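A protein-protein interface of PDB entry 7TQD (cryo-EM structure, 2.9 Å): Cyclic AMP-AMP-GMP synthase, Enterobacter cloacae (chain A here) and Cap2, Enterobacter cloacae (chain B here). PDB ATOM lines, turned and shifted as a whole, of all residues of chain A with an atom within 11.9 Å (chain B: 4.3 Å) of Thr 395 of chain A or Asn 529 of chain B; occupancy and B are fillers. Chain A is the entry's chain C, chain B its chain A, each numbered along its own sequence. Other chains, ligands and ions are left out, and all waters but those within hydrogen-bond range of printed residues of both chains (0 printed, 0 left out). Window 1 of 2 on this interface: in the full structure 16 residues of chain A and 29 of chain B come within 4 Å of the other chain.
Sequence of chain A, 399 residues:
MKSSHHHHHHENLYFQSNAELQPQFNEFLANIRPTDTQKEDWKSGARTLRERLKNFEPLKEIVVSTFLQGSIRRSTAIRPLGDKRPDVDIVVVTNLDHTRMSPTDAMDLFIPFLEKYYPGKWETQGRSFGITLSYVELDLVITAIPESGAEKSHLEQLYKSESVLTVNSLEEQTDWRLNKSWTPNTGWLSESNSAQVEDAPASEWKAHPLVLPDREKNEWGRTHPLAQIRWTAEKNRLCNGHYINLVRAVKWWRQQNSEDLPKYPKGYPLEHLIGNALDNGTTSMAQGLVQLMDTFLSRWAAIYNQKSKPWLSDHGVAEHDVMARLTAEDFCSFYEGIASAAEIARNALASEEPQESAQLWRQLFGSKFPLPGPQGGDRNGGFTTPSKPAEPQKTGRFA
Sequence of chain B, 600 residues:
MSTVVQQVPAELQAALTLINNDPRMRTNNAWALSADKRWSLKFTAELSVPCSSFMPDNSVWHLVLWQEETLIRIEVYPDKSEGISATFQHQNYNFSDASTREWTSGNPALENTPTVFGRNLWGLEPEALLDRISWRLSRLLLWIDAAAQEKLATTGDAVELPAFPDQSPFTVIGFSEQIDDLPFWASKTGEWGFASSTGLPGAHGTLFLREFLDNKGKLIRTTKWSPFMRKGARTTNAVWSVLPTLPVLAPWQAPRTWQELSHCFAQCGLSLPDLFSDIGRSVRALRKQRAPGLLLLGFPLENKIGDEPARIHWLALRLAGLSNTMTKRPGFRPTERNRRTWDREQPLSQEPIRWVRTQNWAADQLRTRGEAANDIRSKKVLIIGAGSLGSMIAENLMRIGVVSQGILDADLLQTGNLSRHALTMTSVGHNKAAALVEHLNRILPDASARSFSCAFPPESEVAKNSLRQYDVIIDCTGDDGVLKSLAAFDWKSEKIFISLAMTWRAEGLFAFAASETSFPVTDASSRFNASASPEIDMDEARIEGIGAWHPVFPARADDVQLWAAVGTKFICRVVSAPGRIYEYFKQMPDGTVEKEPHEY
The guanidinium group of Arg 527 of chain B lies within hydrogen-bond range of the side-chain hydroxyl of Tyr 135 of chain A (3.1 Å). The side-chain amide nitrogen of Asn 529 of chain B lies within hydrogen-bond range of the backbone carbonyl oxygen of Gln 393 of chain A (3.2 Å).
The backbone carbonyl oxygen (O) of Ser 525 of chain B sits close to the side-chain amide oxygen (OD1) of Asn 529 of chain B (3.3 Å).
Among the printed residues, merely in contact across the chains: Thr 395 of chain A with Asn 529 of chain B, Arg 397 of chain A with Phe 528 of chain B, Thr 395 of chain A with Phe 528 of chain B and Thr 395 of chain A with Ser 533 of chain B.
Thr 395 of chain A touches just these residues of chain B: Phe 528 (3.9 Å), Asn 529 (3.5 Å) and Ser 533 (3.9 Å). Of chain A, only Gln 393 (3.2 Å) and Thr 395 (3.5 Å) come within 4 Å of Asn 529 of chain B. No residue of chain A comes within 4 Å of Ser 525 of chain B. No residue of chain A comes within 4 Å of Ser 526 of chain B. Of chain A, only Thr 395 (3.9 Å) and Arg 397 (3.6 Å) come within 4 Å of Phe 528 of chain B. No residue of chain A comes within 4 Å of Ala 530 of chain B. Of chain A, only Thr 395 comes within 4 Å of Ser 533 of chain B. Of the printed residues of chain A, Arg 527 of chain B touches Tyr 135. Printed residues of chain B within 4 Å of Arg 397 of chain A: Phe 528 (3.6 Å). Of the printed residues of chain B, Gln 393 of chain A touches Asn 529. Printed residues of chain B within 4 Å of Tyr 135 of chain A: Arg 527 (3.1 Å). The nearest residue of chain A that does not touch Asn 529 of chain B is Lys 394 of chain A (4.5 Å).
Hydrophobic or aromatic side chains of chain B within 4 Å of the printed part of chain A: Phe 528. Printed residues of chain A that touch a printed residue of chain B: Tyr 135, Gln 393, Thr 395 and Arg 397. Hydrophobic or aromatic side chains of chain A within 4 Å of the printed part of chain B: Tyr 135. Among the printed residues, no Asp or Glu carboxylate lies within 4 Å of a Lys or Arg side-chain nitrogen of the other chain.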
ATOM      1  N   THR A  37       5.193  35.097 -25.879  1.00  0.00           N
ATOM      2  CA  THR A  37       5.626  34.116 -26.869  1.00  0.00           C
ATOM      3  C   THR A  37       6.363  34.792 -28.017  1.00  0.00           C
ATOM      4  O   THR A  37       7.434  34.340 -28.435  1.00  0.00           O
ATOM      5  CB  THR A  37       4.425  33.325 -27.389  1.00  0.00           C
ATOM      6  OG1 THR A  37       3.444  34.230 -27.909  1.00  0.00           O
ATOM      7  CG2 THR A  37       3.804  32.506 -26.272  1.00  0.00           C
ATOM      8  N   TYR A 135       6.315  32.914 -34.958  1.00  0.00           N
ATOM      9  CA  TYR A 135       5.397  33.935 -34.476  1.00  0.00           C
ATOM     10  C   TYR A 135       5.764  35.354 -34.886  1.00  0.00           C
ATOM     11  O   TYR A 135       4.946  36.257 -34.685  1.00  0.00           O
ATOM     12  CB  TYR A 135       5.292  33.885 -32.944  1.00  0.00           C
ATOM     13  CG  TYR A 135       4.785  32.571 -32.401  1.00  0.00           C
ATOM     14  CD1 TYR A 135       3.448  32.221 -32.505  1.00  0.00           C
ATOM     15  CD2 TYR A 135       5.645  31.677 -31.783  1.00  0.00           C
ATOM     16  CE1 TYR A 135       2.983  31.019 -32.008  1.00  0.00           C
ATOM     17  CE2 TYR A 135       5.190  30.473 -31.286  1.00  0.00           C
ATOM     18  CZ  TYR A 135       3.860  30.149 -31.401  1.00  0.00           C
ATOM     19  OH  TYR A 135       3.407  28.951 -30.905  1.00  0.00           O
ATOM     20  N   GLN A 393      -2.873  28.303 -14.875  1.00  0.00           N
ATOM     21  CA  GLN A 393      -3.253  26.931 -15.191  1.00  0.00           C
ATOM     22  C   GLN A 393      -2.049  26.126 -15.664  1.00  0.00           C
ATOM     23  O   GLN A 393      -1.563  26.320 -16.776  1.00  0.00           O
ATOM     24  CB  GLN A 393      -4.352  26.911 -16.256  1.00  0.00           C
ATOM     25  N   LYS A 394      -1.574  25.223 -14.813  1.00  0.00           N
ATOM     26  CA  LYS A 394      -0.431  24.373 -15.119  1.00  0.00           C
ATOM     27  C   LYS A 394      -0.892  22.928 -15.238  1.00  0.00           C
ATOM     28  O   LYS A 394      -1.549  22.404 -14.333  1.00  0.00           O
ATOM     29  CB  LYS A 394       0.648  24.499 -14.044  1.00  0.00           C
ATOM     30  N   THR A 395      -0.548  22.292 -16.354  1.00  0.00           N
ATOM     31  CA  THR A 395      -0.915  20.904 -16.579  1.00  0.00           C
ATOM     32  C   THR A 395       0.017  19.972 -15.811  1.00  0.00           C
ATOM     33  O   THR A 395       1.126  20.341 -15.418  1.00  0.00           O
ATOM     34  CB  THR A 395      -0.878  20.570 -18.069  1.00  0.00           C
ATOM     35  OG1 THR A 395      -1.377  19.243 -18.274  1.00  0.00           O
ATOM     36  CG2 THR A 395       0.541  20.656 -18.598  1.00  0.00           C
ATOM     37  N   GLY A 396      -0.454  18.747 -15.597  1.00  0.00           N
ATOM     38  CA  GLY A 396       0.324  17.759 -14.880  1.00  0.00           C
ATOM     39  C   GLY A 396       1.098  16.827 -15.786  1.00  0.00           C
ATOM     40  O   GLY A 396       0.508  16.075 -16.566  1.00  0.00           O
ATOM     41  N   ARG A 397       2.424  16.872 -15.696  1.00  0.00           N
ATOM     42  CA  ARG A 397       3.300  16.000 -16.462  1.00  0.00           C
ATOM     43  C   ARG A 397       4.127  15.152 -15.507  1.00  0.00           C
ATOM     44  O   ARG A 397       4.682  15.665 -14.531  1.00  0.00           O
ATOM     45  CB  ARG A 397       4.223  16.803 -17.376  1.00  0.00           C
ATOM     46  CG  ARG A 397       3.504  17.778 -18.286  1.00  0.00           C
ATOM     47  CD  ARG A 397       4.488  18.606 -19.086  1.00  0.00           C
ATOM     48  NE  ARG A 397       5.416  19.331 -18.229  1.00  0.00           N
ATOM     49  CZ  ARG A 397       6.731  19.177 -18.252  1.00  0.00           C
ATOM     50  NH1 ARG A 397       7.313  18.326 -19.080  1.00  0.00           N
ATOM     51  NH2 ARG A 397       7.484  19.895 -17.423  1.00  0.00           N
ATOM     52  N   PHE A 398       4.207  13.856 -15.794  1.00  0.00           N
ATOM     53  CA  PHE A 398       4.923  12.909 -14.955  1.00  0.00           C
ATOM     54  C   PHE A 398       5.884  12.100 -15.807  1.00  0.00           C
ATOM     55  O   PHE A 398       5.635  11.861 -16.991  1.00  0.00           O
ATOM     56  CB  PHE A 398       3.961  11.973 -14.225  1.00  0.00           C
ATOM     57  CG  PHE A 398       2.805  12.676 -13.586  1.00  0.00           C
ATOM     58  CD1 PHE A 398       2.916  13.208 -12.318  1.00  0.00           C
ATOM     59  CD2 PHE A 398       1.604  12.809 -14.257  1.00  0.00           C
ATOM     60  CE1 PHE A 398       1.852  13.859 -11.729  1.00  0.00           C
ATOM     61  CE2 PHE A 398       0.537  13.458 -13.672  1.00  0.00           C
ATOM     62  CZ  PHE A 398       0.661  13.984 -12.408  1.00  0.00           C
ATOM     63  N   ALA A 399       6.984  11.676 -15.198  1.00  0.00           N
ATOM     64  CA  ALA A 399       7.995  10.920 -15.921  1.00  0.00           C
ATOM     65  C   ALA A 399       8.775   9.993 -14.998  1.00  0.00           C
ATOM     66  O   ALA A 399       9.413   9.024 -15.404  1.00  0.00           O
ATOM     67  CB  ALA A 399       8.939  11.859 -16.638  1.00  0.00           C
ATOM     68  N   SER B 525       5.057  25.292 -22.830  1.00  0.00           N
ATOM     69  CA  SER B 525       4.006  25.299 -21.820  1.00  0.00           C
ATOM     70  C   SER B 525       2.640  25.530 -22.450  1.00  0.00           C
ATOM     71  O   SER B 525       1.657  24.873 -22.080  1.00  0.00           O
ATOM     72  CB  SER B 525       4.302  26.369 -20.772  1.00  0.00           C
ATOM     73  OG  SER B 525       5.554  26.134 -20.152  1.00  0.00           O
ATOM     74  N   SER B 526       2.556  26.458 -23.405  1.00  0.00           N
ATOM     75  CA  SER B 526       1.286  26.717 -24.074  1.00  0.00           C
ATOM     76  C   SER B 526       0.811  25.494 -24.847  1.00  0.00           C
ATOM     77  O   SER B 526      -0.381  25.168 -24.835  1.00  0.00           O
ATOM     78  CB  SER B 526       1.421  27.920 -25.005  1.00  0.00           C
ATOM     79  OG  SER B 526       0.250  28.083 -25.784  1.00  0.00           O
ATOM     80  N   ARG B 527       1.730  24.807 -25.531  1.00  0.00           N
ATOM     81  CA  ARG B 527       1.351  23.600 -26.261  1.00  0.00           C
ATOM     82  C   ARG B 527       0.874  22.506 -25.315  1.00  0.00           C
ATOM     83  O   ARG B 527      -0.117  21.824 -25.597  1.00  0.00           O
ATOM     84  CB  ARG B 527       2.519  23.108 -27.113  1.00  0.00           C
ATOM     85  CG  ARG B 527       2.917  24.049 -28.240  1.00  0.00           C
ATOM     86  CD  ARG B 527       1.966  23.971 -29.427  1.00  0.00           C
ATOM     87  NE  ARG B 527       0.721  24.697 -29.205  1.00  0.00           N
ATOM     88  CZ  ARG B 527       0.589  26.012 -29.309  1.00  0.00           C
ATOM     89  NH1 ARG B 527       1.614  26.787 -29.622  1.00  0.00           N
ATOM     90  NH2 ARG B 527      -0.600  26.564 -29.093  1.00  0.00           N
ATOM     91  N   PHE B 528       1.565  22.323 -24.186  1.00  0.00           N
ATOM     92  CA  PHE B 528       1.133  21.323 -23.214  1.00  0.00           C
ATOM     93  C   PHE B 528      -0.251  21.645 -22.675  1.00  0.00           C
ATOM     94  O   PHE B 528      -1.085  20.749 -22.507  1.00  0.00           O
ATOM     95  CB  PHE B 528       2.138  21.226 -22.067  1.00  0.00           C
ATOM     96  CG  PHE B 528       3.493  20.745 -22.484  1.00  0.00           C
ATOM     97  CD1 PHE B 528       3.647  19.950 -23.602  1.00  0.00           C
ATOM     98  CD2 PHE B 528       4.615  21.084 -21.751  1.00  0.00           C
ATOM     99  CE1 PHE B 528       4.894  19.507 -23.985  1.00  0.00           C
ATOM    100  CE2 PHE B 528       5.864  20.643 -22.131  1.00  0.00           C
ATOM    101  CZ  PHE B 528       6.003  19.852 -23.249  1.00  0.00           C
ATOM    102  N   ASN B 529      -0.516  22.923 -22.393  1.00  0.00           N
ATOM    103  CA  ASN B 529      -1.822  23.300 -21.864  1.00  0.00           C
ATOM    104  C   ASN B 529      -2.921  23.172 -22.911  1.00  0.00           C
ATOM    105  O   ASN B 529      -4.072  22.889 -22.563  1.00  0.00           O
ATOM    106  CB  ASN B 529      -1.775  24.726 -21.318  1.00  0.00           C
ATOM    107  CG  ASN B 529      -0.786  24.880 -20.180  1.00  0.00           C
ATOM    108  OD1 ASN B 529      -0.297  23.894 -19.631  1.00  0.00           O
ATOM    109  ND2 ASN B 529      -0.486  26.122 -19.821  1.00  0.00           N
ATOM    110  N   ALA B 530      -2.593  23.379 -24.188  1.00  0.00           N
ATOM    111  CA  ALA B 530      -3.618  23.339 -25.227  1.00  0.00           C
ATOM    112  C   ALA B 530      -4.126  21.926 -25.483  1.00  0.00           C
ATOM    113  O   ALA B 530      -5.291  21.748 -25.854  1.00  0.00           O
ATOM    114  CB  ALA B 530      -3.081  23.946 -26.521  1.00  0.00           C
ATOM    115  N   SER B 531      -3.277  20.917 -25.302  1.00  0.00           N
ATOM    116  CA  SER B 531      -3.665  19.543 -25.590  1.00  0.00           C
ATOM    117  C   SER B 531      -4.744  19.064 -24.625  1.00  0.00           C
ATOM    118  O   SER B 531      -4.816  19.494 -23.472  1.00  0.00           O
ATOM    119  CB  SER B 531      -2.451  18.620 -25.509  1.00  0.00           C
ATOM    120  OG  SER B 531      -1.605  18.788 -26.632  1.00  0.00           O
ATOM    121  N   SER B 533      -6.050  16.533 -22.194  1.00  0.00           N
ATOM    122  CA  SER B 533      -5.452  15.541 -21.319  1.00  0.00           C
ATOM    123  C   SER B 533      -6.383  15.241 -20.154  1.00  0.00           C
ATOM    124  O   SER B 533      -7.221  16.074 -19.796  1.00  0.00           O
ATOM    125  CB  SER B 533      -4.096  16.028 -20.788  1.00  0.00           C
ATOM    126  OG  SER B 533      -4.239  17.241 -20.073  1.00  0.00           O
